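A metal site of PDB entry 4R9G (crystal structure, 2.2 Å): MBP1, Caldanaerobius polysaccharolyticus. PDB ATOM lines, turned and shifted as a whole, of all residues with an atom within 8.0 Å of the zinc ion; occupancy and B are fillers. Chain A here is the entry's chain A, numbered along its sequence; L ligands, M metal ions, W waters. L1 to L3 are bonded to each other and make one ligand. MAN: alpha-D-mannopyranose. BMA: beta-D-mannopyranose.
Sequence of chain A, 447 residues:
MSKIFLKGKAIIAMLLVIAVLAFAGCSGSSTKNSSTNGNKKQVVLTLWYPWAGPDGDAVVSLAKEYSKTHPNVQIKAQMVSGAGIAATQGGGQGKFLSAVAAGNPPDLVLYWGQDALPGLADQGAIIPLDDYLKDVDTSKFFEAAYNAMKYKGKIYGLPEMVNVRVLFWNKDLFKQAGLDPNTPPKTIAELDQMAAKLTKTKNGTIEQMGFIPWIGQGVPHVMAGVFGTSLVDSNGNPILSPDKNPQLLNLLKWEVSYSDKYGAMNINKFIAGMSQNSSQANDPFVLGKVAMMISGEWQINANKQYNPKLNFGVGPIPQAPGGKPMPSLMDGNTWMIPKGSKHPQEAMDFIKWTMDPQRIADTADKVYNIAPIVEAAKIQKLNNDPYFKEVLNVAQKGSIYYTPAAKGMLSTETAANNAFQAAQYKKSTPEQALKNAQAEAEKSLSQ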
ATOM      1  N   ALA A  87      30.956 -13.172  24.975  1.00  0.00           N
ATOM      2  CA  ALA A  87      30.854 -13.352  23.515  1.00  0.00           C
ATOM      3  C   ALA A  87      32.193 -13.365  22.764  1.00  0.00           C
ATOM      4  O   ALA A  87      33.058 -12.513  22.993  1.00  0.00           O
ATOM      5  CB  ALA A  87      29.911 -12.303  22.921  1.00  0.00           C
ATOM      6  N   TYR A 111      30.106 -13.251  36.648  1.00  0.00           N
ATOM      7  CA  TYR A 111      30.178 -12.720  35.305  1.00  0.00           C
ATOM      8  C   TYR A 111      30.006 -11.175  35.267  1.00  0.00           C
ATOM      9  O   TYR A 111      29.427 -10.606  36.167  1.00  0.00           O
ATOM     10  CB  TYR A 111      29.157 -13.429  34.430  1.00  0.00           C
ATOM     11  CG  TYR A 111      29.112 -12.931  33.001  1.00  0.00           C
ATOM     12  CD1 TYR A 111      30.217 -13.057  32.165  1.00  0.00           C
ATOM     13  CD2 TYR A 111      27.958 -12.352  32.483  1.00  0.00           C
ATOM     14  CE1 TYR A 111      30.181 -12.614  30.849  1.00  0.00           C
ATOM     15  CE2 TYR A 111      27.906 -11.894  31.160  1.00  0.00           C
ATOM     16  CZ  TYR A 111      29.020 -12.027  30.350  1.00  0.00           C
ATOM     17  OH  TYR A 111      28.966 -11.582  29.048  1.00  0.00           O
ATOM     18  N   TRP A 112      30.516 -10.502  34.244  1.00  0.00           N
ATOM     19  CA  TRP A 112      30.573  -9.042  34.251  1.00  0.00           C
ATOM     20  C   TRP A 112      29.389  -8.355  33.579  1.00  0.00           C
ATOM     21  O   TRP A 112      29.443  -7.148  33.279  1.00  0.00           O
ATOM     22  CB  TRP A 112      31.894  -8.535  33.682  1.00  0.00           C
ATOM     23  CG  TRP A 112      32.181  -8.913  32.250  1.00  0.00           C
ATOM     24  CD1 TRP A 112      31.273  -9.065  31.221  1.00  0.00           C
ATOM     25  CD2 TRP A 112      33.480  -9.136  31.664  1.00  0.00           C
ATOM     26  NE1 TRP A 112      31.925  -9.369  30.053  1.00  0.00           N
ATOM     27  CE2 TRP A 112      33.279  -9.427  30.291  1.00  0.00           C
ATOM     28  CE3 TRP A 112      34.786  -9.109  32.166  1.00  0.00           C
ATOM     29  CZ2 TRP A 112      34.336  -9.702  29.416  1.00  0.00           C
ATOM     30  CZ3 TRP A 112      35.843  -9.384  31.291  1.00  0.00           C
ATOM     31  CH2 TRP A 112      35.609  -9.682  29.934  1.00  0.00           C
ATOM     32  N   GLY A 113      28.321  -9.105  33.354  1.00  0.00           N
ATOM     33  CA  GLY A 113      27.139  -8.568  32.705  1.00  0.00           C
ATOM     34  C   GLY A 113      25.922  -9.407  33.006  1.00  0.00           C
ATOM     35  O   GLY A 113      25.900 -10.148  33.983  1.00  0.00           O
ATOM     36  N   GLN A 114      24.909  -9.293  32.160  1.00  0.00           N
ATOM     37  CA  GLN A 114      23.646  -9.975  32.393  1.00  0.00           C
ATOM     38  C   GLN A 114      23.199 -10.684  31.128  1.00  0.00           C
ATOM     39  O   GLN A 114      22.308 -11.519  31.170  1.00  0.00           O
ATOM     40  CB  GLN A 114      22.564  -8.994  32.852  1.00  0.00           C
ATOM     41  CG  GLN A 114      22.731  -8.467  34.272  1.00  0.00           C
ATOM     42  CD  GLN A 114      21.832  -7.272  34.561  1.00  0.00           C
ATOM     43  OE1 GLN A 114      21.194  -6.734  33.652  1.00  0.00           O
ATOM     44  NE2 GLN A 114      21.793  -6.850  35.820  1.00  0.00           N
ATOM     45  N   ASP A 115      23.847 -10.364  30.012  1.00  0.00           N
ATOM     46  CA  ASP A 115      23.419 -10.813  28.676  1.00  0.00           C
ATOM     47  C   ASP A 115      23.509 -12.317  28.415  1.00  0.00           C
ATOM     48  O   ASP A 115      22.661 -12.873  27.700  1.00  0.00           O
ATOM     49  CB  ASP A 115      24.159 -10.056  27.565  1.00  0.00           C
ATOM     50  CG  ASP A 115      25.659 -10.085  27.712  1.00  0.00           C
ATOM     51  OD1 ASP A 115      26.187 -10.720  28.645  1.00  0.00           O
ATOM     52  OD2 ASP A 115      26.348  -9.464  26.879  1.00  0.00           O
ATOM     53  N   ALA A 116      24.508 -12.970  28.993  1.00  0.00           N
ATOM     54  CA  ALA A 116      24.715 -14.422  28.831  1.00  0.00           C
ATOM     55  C   ALA A 116      23.709 -15.322  29.554  1.00  0.00           C
ATOM     56  O   ALA A 116      23.564 -16.495  29.220  1.00  0.00           O
ATOM     57  CB  ALA A 116      26.124 -14.787  29.263  1.00  0.00           C
ATOM     58  N   ARG A 165      26.243   3.340  32.183  1.00  0.00           N
ATOM     59  CA  ARG A 165      27.161   3.818  31.153  1.00  0.00           C
ATOM     60  C   ARG A 165      27.094   5.341  31.123  1.00  0.00           C
ATOM     61  O   ARG A 165      26.018   5.932  31.223  1.00  0.00           O
ATOM     62  CB  ARG A 165      26.810   3.229  29.812  1.00  0.00           C
ATOM     63  CG  ARG A 165      26.849   1.706  29.760  1.00  0.00           C
ATOM     64  CD  ARG A 165      28.168   1.155  30.287  1.00  0.00           C
ATOM     65  NE  ARG A 165      28.346  -0.248  30.002  1.00  0.00           N
ATOM     66  CZ  ARG A 165      27.863  -1.253  30.727  1.00  0.00           C
ATOM     67  NH1 ARG A 165      27.142  -1.045  31.817  1.00  0.00           N
ATOM     68  NH2 ARG A 165      28.109  -2.498  30.354  1.00  0.00           N
ATOM     69  N   VAL A 219      30.691  -0.050  22.578  1.00  0.00           N
ATOM     70  CA  VAL A 219      30.559  -1.315  21.837  1.00  0.00           C
ATOM     71  C   VAL A 219      29.096  -1.535  21.373  1.00  0.00           C
ATOM     72  O   VAL A 219      28.187  -0.983  21.997  1.00  0.00           O
ATOM     73  CB  VAL A 219      31.093  -2.487  22.694  1.00  0.00           C
ATOM     74  CG1 VAL A 219      32.607  -2.398  22.812  1.00  0.00           C
ATOM     75  CG2 VAL A 219      30.479  -2.465  24.106  1.00  0.00           C
ATOM     76  N   PRO A 220      28.869  -2.318  20.272  1.00  0.00           N
ATOM     77  CA  PRO A 220      27.514  -2.403  19.694  1.00  0.00           C
ATOM     78  C   PRO A 220      26.394  -2.730  20.688  1.00  0.00           C
ATOM     79  O   PRO A 220      25.359  -2.060  20.658  1.00  0.00           O
ATOM     80  CB  PRO A 220      27.637  -3.516  18.646  1.00  0.00           C
ATOM     81  CG  PRO A 220      29.041  -3.378  18.179  1.00  0.00           C
ATOM     82  CD  PRO A 220      29.836  -3.047  19.425  1.00  0.00           C
ATOM     83  N   HIS A 221      26.604  -3.716  21.563  1.00  0.00           N
ATOM     84  CA  HIS A 221      25.576  -4.081  22.557  1.00  0.00           C
ATOM     85  C   HIS A 221      25.223  -2.956  23.565  1.00  0.00           C
ATOM     86  O   HIS A 221      24.148  -3.009  24.164  1.00  0.00           O
ATOM     87  CB  HIS A 221      25.859  -5.451  23.244  1.00  0.00           C
ATOM     88  CG  HIS A 221      26.958  -5.418  24.260  1.00  0.00           C
ATOM     89  ND1 HIS A 221      26.999  -6.284  25.339  1.00  0.00           N
ATOM     90  CD2 HIS A 221      28.054  -4.633  24.378  1.00  0.00           C
ATOM     91  CE1 HIS A 221      28.062  -6.024  26.073  1.00  0.00           C
ATOM     92  NE2 HIS A 221      28.724  -5.025  25.519  1.00  0.00           N
ATOM     93  N   VAL A 222      26.090  -1.952  23.694  1.00  0.00           N
ATOM     94  CA  VAL A 222      25.759  -0.769  24.482  1.00  0.00           C
ATOM     95  C   VAL A 222      25.176   0.295  23.589  1.00  0.00           C
ATOM     96  O   VAL A 222      24.157   0.887  23.900  1.00  0.00           O
ATOM     97  CB  VAL A 222      26.985  -0.197  25.259  1.00  0.00           C
ATOM     98  CG1 VAL A 222      26.777   1.257  25.636  1.00  0.00           C
ATOM     99  CG2 VAL A 222      27.264  -1.001  26.524  1.00  0.00           C
ATOM    100  N   LEU A 231      19.927  -5.276  19.410  1.00  0.00           N
ATOM    101  CA  LEU A 231      20.501  -6.237  18.451  1.00  0.00           C
ATOM    102  C   LEU A 231      19.586  -7.427  18.145  1.00  0.00           C
ATOM    103  O   LEU A 231      19.758  -8.111  17.136  1.00  0.00           O
ATOM    104  CB  LEU A 231      21.895  -6.724  18.888  1.00  0.00           C
ATOM    105  CG  LEU A 231      23.033  -5.716  19.148  1.00  0.00           C
ATOM    106  CD1 LEU A 231      24.227  -6.423  19.812  1.00  0.00           C
ATOM    107  CD2 LEU A 231      23.481  -4.995  17.882  1.00  0.00           C
ATOM    108  N   LEU A 329      22.463   2.420  29.435  1.00  0.00           N
ATOM    109  CA  LEU A 329      22.233   1.033  29.774  1.00  0.00           C
ATOM    110  C   LEU A 329      22.527   0.890  31.260  1.00  0.00           C
ATOM    111  O   LEU A 329      23.585   1.324  31.736  1.00  0.00           O
ATOM    112  CB  LEU A 329      23.174   0.099  28.998  1.00  0.00           C
ATOM    113  CG  LEU A 329      23.200  -1.359  29.544  1.00  0.00           C
ATOM    114  CD1 LEU A 329      21.993  -2.151  29.040  1.00  0.00           C
ATOM    115  CD2 LEU A 329      24.486  -2.073  29.158  1.00  0.00           C
ATOM    116  N   ASP A 331      23.040  -2.189  33.936  1.00  0.00           N
ATOM    117  CA  ASP A 331      23.178  -3.631  34.010  1.00  0.00           C
ATOM    118  C   ASP A 331      23.881  -3.997  35.307  1.00  0.00           C
ATOM    119  O   ASP A 331      23.720  -3.307  36.322  1.00  0.00           O
ATOM    120  CB  ASP A 331      23.926  -4.182  32.781  1.00  0.00           C
ATOM    121  CG  ASP A 331      25.412  -3.792  32.763  1.00  0.00           C
ATOM    122  OD1 ASP A 331      25.819  -2.865  33.518  1.00  0.00           O
ATOM    123  OD2 ASP A 331      26.161  -4.429  31.992  1.00  0.00           O
ATOM    124  N   THR A 403      19.611  -4.732  29.468  1.00  0.00           N
ATOM    125  CA  THR A 403      20.083  -5.821  28.638  1.00  0.00           C
ATOM    126  C   THR A 403      18.849  -6.616  28.233  1.00  0.00           C
ATOM    127  O   THR A 403      18.043  -6.983  29.105  1.00  0.00           O
ATOM    128  CB  THR A 403      21.121  -6.698  29.376  1.00  0.00           C
ATOM    129  OG1 THR A 403      21.346  -7.912  28.644  1.00  0.00           O
ATOM    130  CG2 THR A 403      20.662  -7.046  30.770  1.00  0.00           C
ATOM    131  N   PRO A 404      18.662  -6.838  26.918  1.00  0.00           N
ATOM    132  CA  PRO A 404      17.586  -7.659  26.367  1.00  0.00           C
ATOM    133  C   PRO A 404      17.829  -9.139  26.696  1.00  0.00           C
ATOM    134  O   PRO A 404      18.970  -9.533  26.907  1.00  0.00           O
ATOM    135  CB  PRO A 404      17.684  -7.421  24.844  1.00  0.00           C
ATOM    136  CG  PRO A 404      18.705  -6.333  24.643  1.00  0.00           C
ATOM    137  CD  PRO A 404      19.581  -6.375  25.853  1.00  0.00           C
ATOM    138  N   MET A 409      21.846 -14.328  22.334  1.00  0.00           N
ATOM    139  CA  MET A 409      22.465 -12.987  22.488  1.00  0.00           C
ATOM    140  C   MET A 409      23.965 -12.902  22.146  1.00  0.00           C
ATOM    141  O   MET A 409      24.389 -11.992  21.437  1.00  0.00           O
ATOM    142  CB  MET A 409      22.226 -12.439  23.902  1.00  0.00           C
ATOM    143  CG  MET A 409      22.422 -10.935  24.075  1.00  0.00           C
ATOM    144  SD  MET A 409      21.308  -9.875  23.110  1.00  0.00           S
ATOM    145  CE  MET A 409      22.396  -9.327  21.801  1.00  0.00           C
ATOM    146  N   LEU A 410      24.751 -13.841  22.657  1.00  0.00           N
ATOM    147  CA  LEU A 410      26.206 -13.807  22.468  1.00  0.00           C
ATOM    148  C   LEU A 410      26.688 -14.005  21.029  1.00  0.00           C
ATOM    149  O   LEU A 410      27.589 -13.277  20.554  1.00  0.00           O
ATOM    150  CB  LEU A 410      26.897 -14.809  23.410  1.00  0.00           C
ATOM    151  CG  LEU A 410      27.391 -14.285  24.775  1.00  0.00           C
ATOM    152  CD1 LEU A 410      26.413 -13.325  25.455  1.00  0.00           C
ATOM    153  CD2 LEU A 410      27.718 -15.465  25.671  1.00  0.00           C
ATOM    154  N   GLU A 413      25.762 -10.890  19.091  1.00  0.00           N
ATOM    155  CA  GLU A 413      26.756  -9.875  19.413  1.00  0.00           C
ATOM    156  C   GLU A 413      28.049 -10.072  18.645  1.00  0.00           C
ATOM    157  O   GLU A 413      28.607  -9.094  18.148  1.00  0.00           O
ATOM    158  CB  GLU A 413      27.060  -9.851  20.885  1.00  0.00           C
ATOM    159  CG  GLU A 413      26.111  -8.982  21.685  1.00  0.00           C
ATOM    160  CD  GLU A 413      26.352  -9.092  23.158  1.00  0.00           C
ATOM    161  OE1 GLU A 413      27.519  -9.323  23.578  1.00  0.00           O
ATOM    162  OE2 GLU A 413      25.362  -8.930  23.900  1.00  0.00           O
ATOM    163  N   ASN A 417      29.678  -7.390  16.396  1.00  0.00           N
ATOM    164  CA  ASN A 417      31.025  -6.863  16.623  1.00  0.00           C
ATOM    165  C   ASN A 417      31.896  -6.979  15.382  1.00  0.00           C
ATOM    166  O   ASN A 417      32.623  -6.052  15.025  1.00  0.00           O
ATOM    167  CB  ASN A 417      31.713  -7.557  17.804  1.00  0.00           C
ATOM    168  CG  ASN A 417      31.014  -7.295  19.136  1.00  0.00           C
ATOM    169  OD1 ASN A 417      30.249  -6.331  19.294  1.00  0.00           O
ATOM    170  ND2 ASN A 417      31.300  -8.138  20.107  1.00  0.00           N
HETATM  171  C1  MAN L   1      32.968  -6.741  24.159  1.00  0.00           C
HETATM  172  C2  MAN L   1      31.883  -6.869  25.223  1.00  0.00           C
HETATM  173  C3  MAN L   1      32.298  -6.185  26.537  1.00  0.00           C
HETATM  174  C4  MAN L   1      33.767  -6.387  26.924  1.00  0.00           C
HETATM  175  C5  MAN L   1      34.662  -6.333  25.687  1.00  0.00           C
HETATM  176  C6  MAN L   1      36.107  -6.699  25.980  1.00  0.00           C
HETATM  177  O1  MAN L   1      33.109  -5.372  23.851  1.00  0.00           O
HETATM  178  O2  MAN L   1      31.681  -8.244  25.465  1.00  0.00           O
HETATM  179  O3  MAN L   1      31.470  -6.717  27.542  1.00  0.00           O
HETATM  180  O4  MAN L   1      34.215  -5.379  27.808  1.00  0.00           O
HETATM  181  O5  MAN L   1      34.167  -7.208  24.699  1.00  0.00           O
HETATM  182  O6  MAN L   1      36.082  -7.749  26.895  1.00  0.00           O
HETATM  183  C1  BMA L   2      33.868  -5.643  29.188  1.00  0.00           C
HETATM  184  C2  BMA L   2      34.985  -5.169  30.104  1.00  0.00           C
HETATM  185  C3  BMA L   2      34.564  -5.374  31.575  1.00  0.00           C
HETATM  186  C4  BMA L   2      33.237  -4.702  31.902  1.00  0.00           C
HETATM  187  C5  BMA L   2      32.192  -5.204  30.896  1.00  0.00           C
HETATM  188  C6  BMA L   2      30.863  -4.491  31.112  1.00  0.00           C
HETATM  189  O2  BMA L   2      35.233  -3.790  29.841  1.00  0.00           O
HETATM  190  O3  BMA L   2      35.613  -4.989  32.482  1.00  0.00           O
HETATM  191  O4  BMA L   2      32.776  -5.123  33.186  1.00  0.00           O
HETATM  192  O5  BMA L   2      32.626  -5.007  29.556  1.00  0.00           O
HETATM  193  O6  BMA L   2      29.830  -5.125  30.350  1.00  0.00           O
HETATM  194  C1  BMA L   3      32.900  -4.123  34.184  1.00  0.00           C
HETATM  195  C2  BMA L   3      31.952  -4.461  35.334  1.00  0.00           C
HETATM  196  C3  BMA L   3      32.165  -3.572  36.550  1.00  0.00           C
HETATM  197  C4  BMA L   3      33.650  -3.556  36.918  1.00  0.00           C
HETATM  198  C5  BMA L   3      34.556  -3.265  35.730  1.00  0.00           C
HETATM  199  C6  BMA L   3      36.024  -3.518  36.112  1.00  0.00           C
HETATM  200  O2  BMA L   3      32.152  -5.816  35.754  1.00  0.00           O
HETATM  201  O3  BMA L   3      31.410  -4.086  37.651  1.00  0.00           O
HETATM  202  O4  BMA L   3      33.880  -2.569  37.924  1.00  0.00           O
HETATM  203  O5  BMA L   3      34.249  -4.125  34.627  1.00  0.00           O
HETATM  204  O6  BMA L   3      36.780  -3.133  34.978  1.00  0.00           O
HETATM  205 ZN    ZN M   1      25.744  -7.891  25.680  1.00  0.00          ZN
HETATM  206  O   HOH W   1      24.521  -6.511  27.195  1.00  0.00           O
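NH2 of Arg 165 is in hydrogen-bond range of O6 of BMA L2 (3.1 Å).
The backbone carbonyl oxygen (O) of Glu 413 lies close to the side-chain amide oxygen (OD1) of Asn 417. The side-chain carboxylate (OD1) of Asp 115 lies within hydrogen-bond range of the side-chain hydroxyl (OH) of Tyr 111 (2.9 Å).
Of the 21 residues printed, 3 come within 4 Å of the zinc ion. The nearest printed residue that does not touch the zinc ion is Met 409 (4.8 Å).
The zinc ion is bound by ND1 of His 221 (2.1 Å), OD2 of Asp 115 (2.1 Å), OE2 of Glu 413 (2.1 Å) and water W1 (2.4 Å). The zinc ion has four donor atoms within binding distance.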
